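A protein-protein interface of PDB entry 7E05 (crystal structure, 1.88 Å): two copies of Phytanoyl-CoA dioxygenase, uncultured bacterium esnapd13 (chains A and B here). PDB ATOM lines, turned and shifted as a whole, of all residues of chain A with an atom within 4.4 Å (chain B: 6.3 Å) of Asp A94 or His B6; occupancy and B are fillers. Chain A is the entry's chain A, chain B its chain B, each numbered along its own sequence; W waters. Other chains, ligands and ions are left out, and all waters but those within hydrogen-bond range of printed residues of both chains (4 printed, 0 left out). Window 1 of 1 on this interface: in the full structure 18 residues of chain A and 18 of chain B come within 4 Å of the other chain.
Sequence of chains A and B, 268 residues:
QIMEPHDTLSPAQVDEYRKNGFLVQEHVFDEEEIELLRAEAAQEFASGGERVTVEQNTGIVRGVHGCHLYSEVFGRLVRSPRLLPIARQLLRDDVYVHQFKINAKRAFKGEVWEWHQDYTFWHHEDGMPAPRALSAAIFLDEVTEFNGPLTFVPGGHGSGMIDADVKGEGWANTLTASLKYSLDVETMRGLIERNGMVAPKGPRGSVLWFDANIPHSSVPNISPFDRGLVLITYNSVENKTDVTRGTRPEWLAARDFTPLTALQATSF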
ATOM      1  N   ARG A  88     -18.642 -35.124  29.279  1.00  0.00           N
ATOM      2  CA  ARG A  88     -18.956 -33.946  28.444  1.00  0.00           C
ATOM      3  C   ARG A  88     -17.838 -32.974  28.296  1.00  0.00           C
ATOM      4  O   ARG A  88     -17.540 -32.505  27.189  1.00  0.00           O
ATOM      5  CB  ARG A  88     -20.174 -33.229  29.024  1.00  0.00           C
ATOM      6  CG  ARG A  88     -21.481 -33.975  28.898  1.00  0.00           C
ATOM      7  CD  ARG A  88     -22.529 -33.113  29.640  1.00  0.00           C
ATOM      8  NE  ARG A  88     -23.900 -33.558  29.425  1.00  0.00           N
ATOM      9  CZ  ARG A  88     -24.960 -32.954  29.977  1.00  0.00           C
ATOM     10  NH1 ARG A  88     -24.797 -31.913  30.749  1.00  0.00           N
ATOM     11  NH2 ARG A  88     -26.184 -33.354  29.741  1.00  0.00           N
ATOM     12  N   ARG A  92     -15.824 -32.744  24.930  1.00  0.00           N
ATOM     13  CA  ARG A  92     -16.234 -31.448  24.497  1.00  0.00           C
ATOM     14  C   ARG A  92     -17.507 -31.552  23.611  1.00  0.00           C
ATOM     15  O   ARG A  92     -17.600 -31.004  22.538  1.00  0.00           O
ATOM     16  CB  ARG A  92     -15.087 -30.746  23.750  1.00  0.00           C
ATOM     17  CG  ARG A  92     -13.794 -30.563  24.586  1.00  0.00           C
ATOM     18  CD  ARG A  92     -12.636 -30.092  23.708  1.00  0.00           C
ATOM     19  NE  ARG A  92     -12.901 -28.695  23.460  1.00  0.00           N
ATOM     20  CZ  ARG A  92     -12.060 -27.839  22.827  1.00  0.00           C
ATOM     21  NH1 ARG A  92     -10.850 -28.252  22.337  1.00  0.00           N
ATOM     22  NH2 ARG A  92     -12.454 -26.576  22.641  1.00  0.00           N
ATOM     23  N   ASP A  93     -18.463 -32.285  24.076  1.00  0.00           N
ATOM     24  CA  ASP A  93     -19.717 -32.480  23.355  1.00  0.00           C
ATOM     25  C   ASP A  93     -20.717 -33.012  24.305  1.00  0.00           C
ATOM     26  O   ASP A  93     -20.428 -33.393  25.467  1.00  0.00           O
ATOM     27  CB  ASP A  93     -19.459 -33.590  22.272  1.00  0.00           C
ATOM     28  CG  ASP A  93     -20.461 -33.603  21.173  1.00  0.00           C
ATOM     29  OD1 ASP A  93     -21.436 -32.749  21.160  1.00  0.00           O
ATOM     30  OD2 ASP A  93     -20.319 -34.494  20.268  1.00  0.00           O
ATOM     31  N   ASP A  94     -21.936 -33.130  23.835  1.00  0.00           N
ATOM     32  CA  ASP A  94     -22.847 -33.991  24.484  1.00  0.00           C
ATOM     33  C   ASP A  94     -22.365 -35.465  24.183  1.00  0.00           C
ATOM     34  O   ASP A  94     -21.698 -35.743  23.230  1.00  0.00           O
ATOM     35  CB  ASP A  94     -24.236 -33.925  23.893  1.00  0.00           C
ATOM     36  CG  ASP A  94     -25.145 -32.899  24.577  1.00  0.00           C
ATOM     37  OD1 ASP A  94     -25.094 -32.733  25.846  1.00  0.00           O
ATOM     38  OD2 ASP A  94     -25.990 -32.376  23.772  1.00  0.00           O
ATOM     39  N   VAL A  95     -22.770 -36.370  25.047  1.00  0.00           N
ATOM     40  CA  VAL A  95     -22.361 -37.748  24.967  1.00  0.00           C
ATOM     41  C   VAL A  95     -23.453 -38.749  25.166  1.00  0.00           C
ATOM     42  O   VAL A  95     -24.498 -38.472  25.699  1.00  0.00           O
ATOM     43  CB  VAL A  95     -21.273 -38.037  26.064  1.00  0.00           C
ATOM     44  CG1 VAL A  95     -20.010 -37.173  25.873  1.00  0.00           C
ATOM     45  CG2 VAL A  95     -21.776 -37.799  27.459  1.00  0.00           C
ATOM     46  N   ASN A 235     -19.164 -41.861  24.316  1.00  0.00           N
ATOM     47  CA  ASN A 235     -18.766 -41.405  23.022  1.00  0.00           C
ATOM     48  C   ASN A 235     -19.387 -40.063  22.774  1.00  0.00           C
ATOM     49  O   ASN A 235     -20.534 -39.780  23.198  1.00  0.00           O
ATOM     50  CB  ASN A 235     -19.145 -42.445  21.934  1.00  0.00           C
ATOM     51  CG  ASN A 235     -18.559 -42.070  20.554  1.00  0.00           C
ATOM     52  OD1 ASN A 235     -17.586 -41.366  20.452  1.00  0.00           O
ATOM     53  ND2 ASN A 235     -19.160 -42.589  19.493  1.00  0.00           N
ATOM     54  N   SER A 236     -18.668 -39.195  22.078  1.00  0.00           N
ATOM     55  CA  SER A 236     -19.223 -37.934  21.575  1.00  0.00           C
ATOM     56  C   SER A 236     -20.406 -38.195  20.667  1.00  0.00           C
ATOM     57  O   SER A 236     -20.362 -39.092  19.799  1.00  0.00           O
ATOM     58  CB  SER A 236     -18.092 -37.165  20.827  1.00  0.00           C
ATOM     59  OG  SER A 236     -18.659 -36.347  19.767  1.00  0.00           O
ATOM     60  N   VAL A 237     -21.483 -37.449  20.818  1.00  0.00           N
ATOM     61  CA  VAL A 237     -22.659 -37.573  19.926  1.00  0.00           C
ATOM     62  C   VAL A 237     -22.334 -37.209  18.497  1.00  0.00           C
ATOM     63  O   VAL A 237     -22.747 -37.922  17.551  1.00  0.00           O
ATOM     64  CB  VAL A 237     -23.811 -36.696  20.466  1.00  0.00           C
ATOM     65  CG1 VAL A 237     -25.014 -36.543  19.552  1.00  0.00           C
ATOM     66  CG2 VAL A 237     -24.349 -37.279  21.781  1.00  0.00           C
ATOM     67  N   PRO A 259     -28.655 -37.704  23.425  1.00  0.00           N
ATOM     68  CA  PRO A 259     -27.685 -37.183  24.374  1.00  0.00           C
ATOM     69  C   PRO A 259     -28.172 -37.491  25.778  1.00  0.00           C
ATOM     70  O   PRO A 259     -29.373 -37.268  26.140  1.00  0.00           O
ATOM     71  CB  PRO A 259     -27.673 -35.660  24.122  1.00  0.00           C
ATOM     72  CG  PRO A 259     -28.165 -35.520  22.807  1.00  0.00           C
ATOM     73  CD  PRO A 259     -29.116 -36.658  22.517  1.00  0.00           C
ATOM     74  N   MET B   3     -19.513 -29.593  14.241  1.00  0.00           N
ATOM     75  CA  MET B   3     -19.504 -28.394  15.060  1.00  0.00           C
ATOM     76  C   MET B   3     -18.108 -28.262  15.670  1.00  0.00           C
ATOM     77  O   MET B   3     -17.496 -29.257  16.096  1.00  0.00           O
ATOM     78  CB  MET B   3     -20.560 -28.358  16.223  1.00  0.00           C
ATOM     79  CG  MET B   3     -21.988 -28.342  15.792  1.00  0.00           C
ATOM     80  SD  MET B   3     -22.341 -26.680  15.140  1.00  0.00           S
ATOM     81  CE  MET B   3     -24.135 -26.630  15.262  1.00  0.00           C
ATOM     82  N   GLU B   4     -17.679 -27.038  15.858  1.00  0.00           N
ATOM     83  CA  GLU B   4     -16.462 -26.816  16.614  1.00  0.00           C
ATOM     84  C   GLU B   4     -16.654 -27.437  18.021  1.00  0.00           C
ATOM     85  O   GLU B   4     -17.750 -27.253  18.629  1.00  0.00           O
ATOM     86  CB  GLU B   4     -16.160 -25.340  16.803  1.00  0.00           C
ATOM     87  CG  GLU B   4     -15.634 -24.691  15.531  1.00  0.00           C
ATOM     88  CD  GLU B   4     -15.794 -23.165  15.596  1.00  0.00           C
ATOM     89  OE1 GLU B   4     -15.328 -22.588  16.616  1.00  0.00           O
ATOM     90  OE2 GLU B   4     -16.451 -22.561  14.691  1.00  0.00           O
ATOM     91  N   PRO B   5     -15.650 -28.148  18.494  1.00  0.00           N
ATOM     92  CA  PRO B   5     -15.854 -28.752  19.840  1.00  0.00           C
ATOM     93  C   PRO B   5     -16.202 -27.717  20.875  1.00  0.00           C
ATOM     94  O   PRO B   5     -15.763 -26.612  20.750  1.00  0.00           O
ATOM     95  CB  PRO B   5     -14.502 -29.414  20.134  1.00  0.00           C
ATOM     96  CG  PRO B   5     -13.874 -29.676  18.791  1.00  0.00           C
ATOM     97  CD  PRO B   5     -14.370 -28.564  17.876  1.00  0.00           C
ATOM     98  N   HIS B   6     -16.995 -28.065  21.883  1.00  0.00           N
ATOM     99  CA  HIS B   6     -17.483 -27.107  22.840  1.00  0.00           C
ATOM    100  C   HIS B   6     -16.324 -26.410  23.550  1.00  0.00           C
ATOM    101  O   HIS B   6     -15.304 -27.048  23.909  1.00  0.00           O
ATOM    102  CB  HIS B   6     -18.353 -27.808  23.889  1.00  0.00           C
ATOM    103  CG  HIS B   6     -19.595 -28.417  23.326  1.00  0.00           C
ATOM    104  ND1 HIS B   6     -20.439 -29.155  24.094  1.00  0.00           N
ATOM    105  CD2 HIS B   6     -20.202 -28.273  22.124  1.00  0.00           C
ATOM    106  CE1 HIS B   6     -21.482 -29.518  23.382  1.00  0.00           C
ATOM    107  NE2 HIS B   6     -21.354 -29.021  22.171  1.00  0.00           N
ATOM    108  N   ASP B   7     -16.461 -25.091  23.603  1.00  0.00           N
ATOM    109  CA  ASP B   7     -15.473 -24.177  24.207  1.00  0.00           C
ATOM    110  C   ASP B   7     -16.067 -23.647  25.497  1.00  0.00           C
ATOM    111  O   ASP B   7     -17.110 -23.079  25.421  1.00  0.00           O
ATOM    112  CB  ASP B   7     -15.280 -22.961  23.315  1.00  0.00           C
ATOM    113  CG  ASP B   7     -13.899 -22.933  22.745  1.00  0.00           C
ATOM    114  OD1 ASP B   7     -13.580 -23.860  22.033  1.00  0.00           O
ATOM    115  OD2 ASP B   7     -13.163 -21.986  23.045  1.00  0.00           O
ATOM    116  N   THR B   8     -15.457 -23.910  26.629  1.00  0.00           N
ATOM    117  CA  THR B   8     -16.012 -23.373  27.852  1.00  0.00           C
ATOM    118  C   THR B   8     -15.149 -22.198  28.310  1.00  0.00           C
ATOM    119  O   THR B   8     -14.074 -21.939  27.722  1.00  0.00           O
ATOM    120  CB  THR B   8     -16.011 -24.507  28.870  1.00  0.00           C
ATOM    121  OG1 THR B   8     -14.784 -25.207  28.757  1.00  0.00           O
ATOM    122  CG2 THR B   8     -17.202 -25.488  28.531  1.00  0.00           C
ATOM    123  N   PRO B  81     -23.938 -24.510  20.401  1.00  0.00           N
ATOM    124  CA  PRO B  81     -22.736 -24.879  21.123  1.00  0.00           C
ATOM    125  C   PRO B  81     -21.926 -23.695  21.534  1.00  0.00           C
ATOM    126  O   PRO B  81     -21.021 -23.884  22.264  1.00  0.00           O
ATOM    127  CB  PRO B  81     -21.965 -25.746  20.117  1.00  0.00           C
ATOM    128  CG  PRO B  81     -22.486 -25.342  18.783  1.00  0.00           C
ATOM    129  CD  PRO B  81     -23.973 -25.052  19.046  1.00  0.00           C
ATOM    130  N   ARG B  82     -22.265 -22.497  21.096  1.00  0.00           N
ATOM    131  CA  ARG B  82     -21.592 -21.317  21.632  1.00  0.00           C
ATOM    132  C   ARG B  82     -22.105 -20.892  22.993  1.00  0.00           C
ATOM    133  O   ARG B  82     -21.524 -19.953  23.587  1.00  0.00           O
ATOM    134  CB  ARG B  82     -21.741 -20.106  20.714  1.00  0.00           C
ATOM    135  CG  ARG B  82     -21.335 -20.293  19.295  1.00  0.00           C
ATOM    136  CD  ARG B  82     -19.883 -20.493  19.135  1.00  0.00           C
ATOM    137  NE  ARG B  82     -19.581 -20.290  17.709  1.00  0.00           N
ATOM    138  CZ  ARG B  82     -18.521 -20.874  17.117  1.00  0.00           C
ATOM    139  NH1 ARG B  82     -17.735 -21.672  17.835  1.00  0.00           N
ATOM    140  NH2 ARG B  82     -18.265 -20.703  15.801  1.00  0.00           N
ATOM    141  N   LEU B  84     -24.759 -23.040  25.130  1.00  0.00           N
ATOM    142  CA  LEU B  84     -25.220 -24.001  26.092  1.00  0.00           C
ATOM    143  C   LEU B  84     -24.116 -24.529  26.965  1.00  0.00           C
ATOM    144  O   LEU B  84     -24.338 -24.739  28.172  1.00  0.00           O
ATOM    145  CB  LEU B  84     -25.997 -25.130  25.337  1.00  0.00           C
ATOM    146  CG  LEU B  84     -26.521 -26.232  26.225  1.00  0.00           C
ATOM    147  CD1 LEU B  84     -27.558 -25.660  27.163  1.00  0.00           C
ATOM    148  CD2 LEU B  84     -27.133 -27.348  25.385  1.00  0.00           C
ATOM    149  N   PRO B  85     -22.948 -24.853  26.440  1.00  0.00           N
ATOM    150  CA  PRO B  85     -21.960 -25.404  27.298  1.00  0.00           C
ATOM    151  C   PRO B  85     -21.462 -24.485  28.408  1.00  0.00           C
ATOM    152  O   PRO B  85     -21.104 -24.952  29.510  1.00  0.00           O
ATOM    153  CB  PRO B  85     -20.781 -25.716  26.344  1.00  0.00           C
ATOM    154  CG  PRO B  85     -21.444 -25.949  25.046  1.00  0.00           C
ATOM    155  CD  PRO B  85     -22.523 -24.930  25.046  1.00  0.00           C
ATOM    156  N   ARG B  88     -24.187 -24.376  31.112  1.00  0.00           N
ATOM    157  CA  ARG B  88     -24.102 -25.552  32.008  1.00  0.00           C
ATOM    158  C   ARG B  88     -22.874 -25.503  32.945  1.00  0.00           C
ATOM    159  O   ARG B  88     -22.864 -25.936  34.087  1.00  0.00           O
ATOM    160  CB  ARG B  88     -23.883 -26.768  31.092  1.00  0.00           C
ATOM    161  CG  ARG B  88     -25.063 -27.278  30.274  1.00  0.00           C
ATOM    162  CD  ARG B  88     -24.598 -28.359  29.304  1.00  0.00           C
ATOM    163  NE  ARG B  88     -25.702 -29.064  28.635  1.00  0.00           N
ATOM    164  CZ  ARG B  88     -25.516 -30.053  27.796  1.00  0.00           C
ATOM    165  NH1 ARG B  88     -24.286 -30.454  27.476  1.00  0.00           N
ATOM    166  NH2 ARG B  88     -26.557 -30.685  27.275  1.00  0.00           N
ATOM    167  N   ASP B  94     -27.364 -29.328  34.285  1.00  0.00           N
ATOM    168  CA  ASP B  94     -28.087 -29.180  33.111  1.00  0.00           C
ATOM    169  C   ASP B  94     -29.006 -27.921  33.263  1.00  0.00           C
ATOM    170  O   ASP B  94     -29.285 -27.466  34.403  1.00  0.00           O
ATOM    171  CB  ASP B  94     -29.036 -30.363  32.922  1.00  0.00           C
ATOM    172  CG  ASP B  94     -28.418 -31.505  32.146  1.00  0.00           C
ATOM    173  OD1 ASP B  94     -27.593 -31.254  31.211  1.00  0.00           O
ATOM    174  OD2 ASP B  94     -28.890 -32.691  32.356  1.00  0.00           O
ATOM    175  N   LEU B 260     -31.834 -29.015  28.191  1.00  0.00           N
ATOM    176  CA  LEU B 260     -31.417 -28.763  26.815  1.00  0.00           C
ATOM    177  C   LEU B 260     -30.198 -29.578  26.399  1.00  0.00           C
ATOM    178  O   LEU B 260     -29.335 -29.821  27.199  1.00  0.00           O
ATOM    179  CB  LEU B 260     -31.046 -27.267  26.628  1.00  0.00           C
ATOM    180  CG  LEU B 260     -32.214 -26.319  26.759  1.00  0.00           C
ATOM    181  CD1 LEU B 260     -31.674 -24.940  26.874  1.00  0.00           C
ATOM    182  CD2 LEU B 260     -33.125 -26.331  25.586  1.00  0.00           C
ATOM    183  N   THR B 261     -30.220 -29.998  25.112  1.00  0.00           N
ATOM    184  CA  THR B 261     -29.111 -30.616  24.438  1.00  0.00           C
ATOM    185  C   THR B 261     -28.533 -29.712  23.370  1.00  0.00           C
ATOM    186  O   THR B 261     -29.229 -28.884  22.806  1.00  0.00           O
ATOM    187  CB  THR B 261     -29.604 -31.957  23.710  1.00  0.00           C
ATOM    188  OG1 THR B 261     -30.340 -31.592  22.509  1.00  0.00           O
ATOM    189  CG2 THR B 261     -30.419 -32.709  24.586  1.00  0.00           C
ATOM    190  N   ALA B 262     -27.277 -29.875  23.069  1.00  0.00           N
ATOM    191  CA  ALA B 262     -26.597 -29.033  22.130  1.00  0.00           C
ATOM    192  C   ALA B 262     -27.015 -29.388  20.708  1.00  0.00           C
ATOM    193  O   ALA B 262     -27.320 -30.558  20.381  1.00  0.00           O
ATOM    194  CB  ALA B 262     -25.113 -29.217  22.220  1.00  0.00           C
ATOM    195  N   LEU B 263     -27.019 -28.359  19.870  1.00  0.00           N
ATOM    196  CA  LEU B 263     -27.347 -28.506  18.451  1.00  0.00           C
ATOM    197  C   LEU B 263     -26.173 -29.237  17.787  1.00  0.00           C
ATOM    198  O   LEU B 263     -25.005 -28.910  18.110  1.00  0.00           O
ATOM    199  CB  LEU B 263     -27.450 -27.094  17.929  1.00  0.00           C
ATOM    200  CG  LEU B 263     -28.090 -26.856  16.631  1.00  0.00           C
ATOM    201  CD1 LEU B 263     -29.557 -27.312  16.683  1.00  0.00           C
ATOM    202  CD2 LEU B 263     -27.892 -25.354  16.343  1.00  0.00           C
ATOM    203  N   GLN B 264     -26.442 -30.324  17.023  1.00  0.00           N
ATOM    204  CA  GLN B 264     -25.361 -30.970  16.237  1.00  0.00           C
ATOM    205  C   GLN B 264     -25.294 -30.418  14.784  1.00  0.00           C
ATOM    206  O   GLN B 264     -26.259 -29.788  14.340  1.00  0.00           O
ATOM    207  CB  GLN B 264     -25.556 -32.465  16.230  1.00  0.00           C
ATOM    208  CG  GLN B 264     -25.408 -33.096  17.646  1.00  0.00           C
ATOM    209  CD  GLN B 264     -23.995 -32.974  18.246  1.00  0.00           C
ATOM    210  OE1 GLN B 264     -23.011 -32.844  17.536  1.00  0.00           O
ATOM    211  NE2 GLN B 264     -23.907 -33.028  19.604  1.00  0.00           N
HETATM  212  O   HOH W   1     -20.968 -31.399  18.740  1.00  0.00           O
HETATM  213  O   HOH W   2     -13.547 -25.442  19.691  1.00  0.00           O
HETATM  214  O   HOH W   3     -19.658 -30.294  26.475  1.00  0.00           O
HETATM  215  O   HOH W   4     -26.494 -32.968  21.116  1.00  0.00           O
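Arg A88 touches its own counterpart, Arg B88.
Arg A88 touches Asp B94, and with the chains exchanged Asp A94 touches Arg B88.
N of Asp A93 is in hydrogen-bond range of O of Arg A88, at 3.3 Å.
The side-chain carboxylate (OD2) of Asp A93 lies within hydrogen-bond range of the side-chain hydroxyl (OG) of Ser A236 (2.5 Å).
The side-chain carboxylate (OD2) of Asp A93 lies within hydrogen-bond range of the backbone NH (N) of Val A237.
The backbone NH (N) of Val A237 sits at hydrogen-bond distance from the backbone carbonyl oxygen (O) of Asp A94, 3.0 Å away.
The side-chain carboxylate of Asp B94 lies within salt-bridge range of the guanidinium group of Arg B88, at 3.9 Å.
The backbone carbonyl oxygen (O) of Leu B260 sits at hydrogen-bond distance from the guanidinium group (NH2) of Arg B88 (2.9 Å).
Of the printed residues of chain B, Asp A93 touches His B6 and Gln B264.
Asp A94 touches just these residues of chain B: His B6 (3.7 Å), Arg B88 (2.9 Å), Thr B261 (3.6 Å) and Ala B262 (2.9 Å).
Printed residues of chain B within 4 Å of Pro A259: Thr B261.
Printed residues of chain A within 4 Å of Pro B5: Arg A92.
Of chain A, only Arg A92 (2.9 Å), Asp A93 (3.4 Å) and Asp A94 (3.7 Å) come within 4 Å of His B6.
Printed residues of chain A within 4 Å of Asp B94: Arg A88.
The nearest printed residue of chain A that does not touch His B6 is Arg A88 (5.4 Å).
The nearest printed residue of chain A that does not touch Asp B7 is Asp A93 (7.5 Å).
Water W4 lies within hydrogen-bond range of the backbone carbonyl oxygen of Ala B262, the side-chain carboxylate of Asp A94 and the side-chain amide nitrogen of Gln B264.
Water W2 lies within hydrogen-bond range of O of Pro B5, OD1 of Asp B7 and NH2 of Arg A92.
Water W3 lies within hydrogen-bond range of a ring nitrogen (ND1) of His B6, the backbone carbonyl oxygen (O) of Arg A88 and the backbone NH (N) of Asp A93.
Water W1 lies within hydrogen-bond range of the side-chain amide oxygen (OE1) of Gln B264 (2.8 Å) and the side-chain carboxylate (OD1) of Asp A93 (2.8 Å).
The guanidinium group of Arg A88 is in salt-bridge range of the side-chain carboxylate of Asp B94 (2.9 Å).
The backbone carbonyl oxygen of His B6 is in hydrogen-bond range of the guanidinium group of Arg A92, 2.9 Å away.
NH2 of Arg A92 is in salt-bridge range of OD1 of Asp B7, at 3.0 Å.
OD1 of Asp A93 is in hydrogen-bond range of NE2 of Gln B264 (2.9 Å).
The side-chain carboxylate (OD1) of Asp A94 is in salt-bridge range of the guanidinium group (NH2) of Arg B88 (2.9 Å).
The backbone NH (N) of Ala B262 is in hydrogen-bond range of the side-chain carboxylate (OD2) of Asp A94, at 2.9 Å.
Hydrophobic or aromatic side chains of chain A within 4 Å of the printed part of chain B: Val A237 and Pro A259.
Hydrophobic or aromatic side chains of chain B that line the printed part of chain A: Pro B5, His B6 and Ala B262.
Among the printed residues, 13 pairs touch across the chains.
Among the printed residues, Asp or Glu carboxylates within 4 Å of a Lys or Arg side-chain nitrogen of the other chain: Arg A88 with Asp B94 (2.9 Å), Arg A92 with Asp B7 (3.0 Å) and Asp A94 with Arg B88 (2.9 Å).
Arg A88 touches Arg B88 (NH1 to CZ, 3.6 Å).
Arg A92 touches Pro B5.
Asp A93 touches His B6 (CA to CE1, 3.4 Å).
N of Asp A94 touches CE1 of His B6, 3.7 Å away.
Asp A94 touches Thr B261 (OD2 to CB, 3.6 Å).
Gln B264 touches Val A237 (NE2 to CG1, 3.7 Å).
Pro A259 touches Thr B261.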
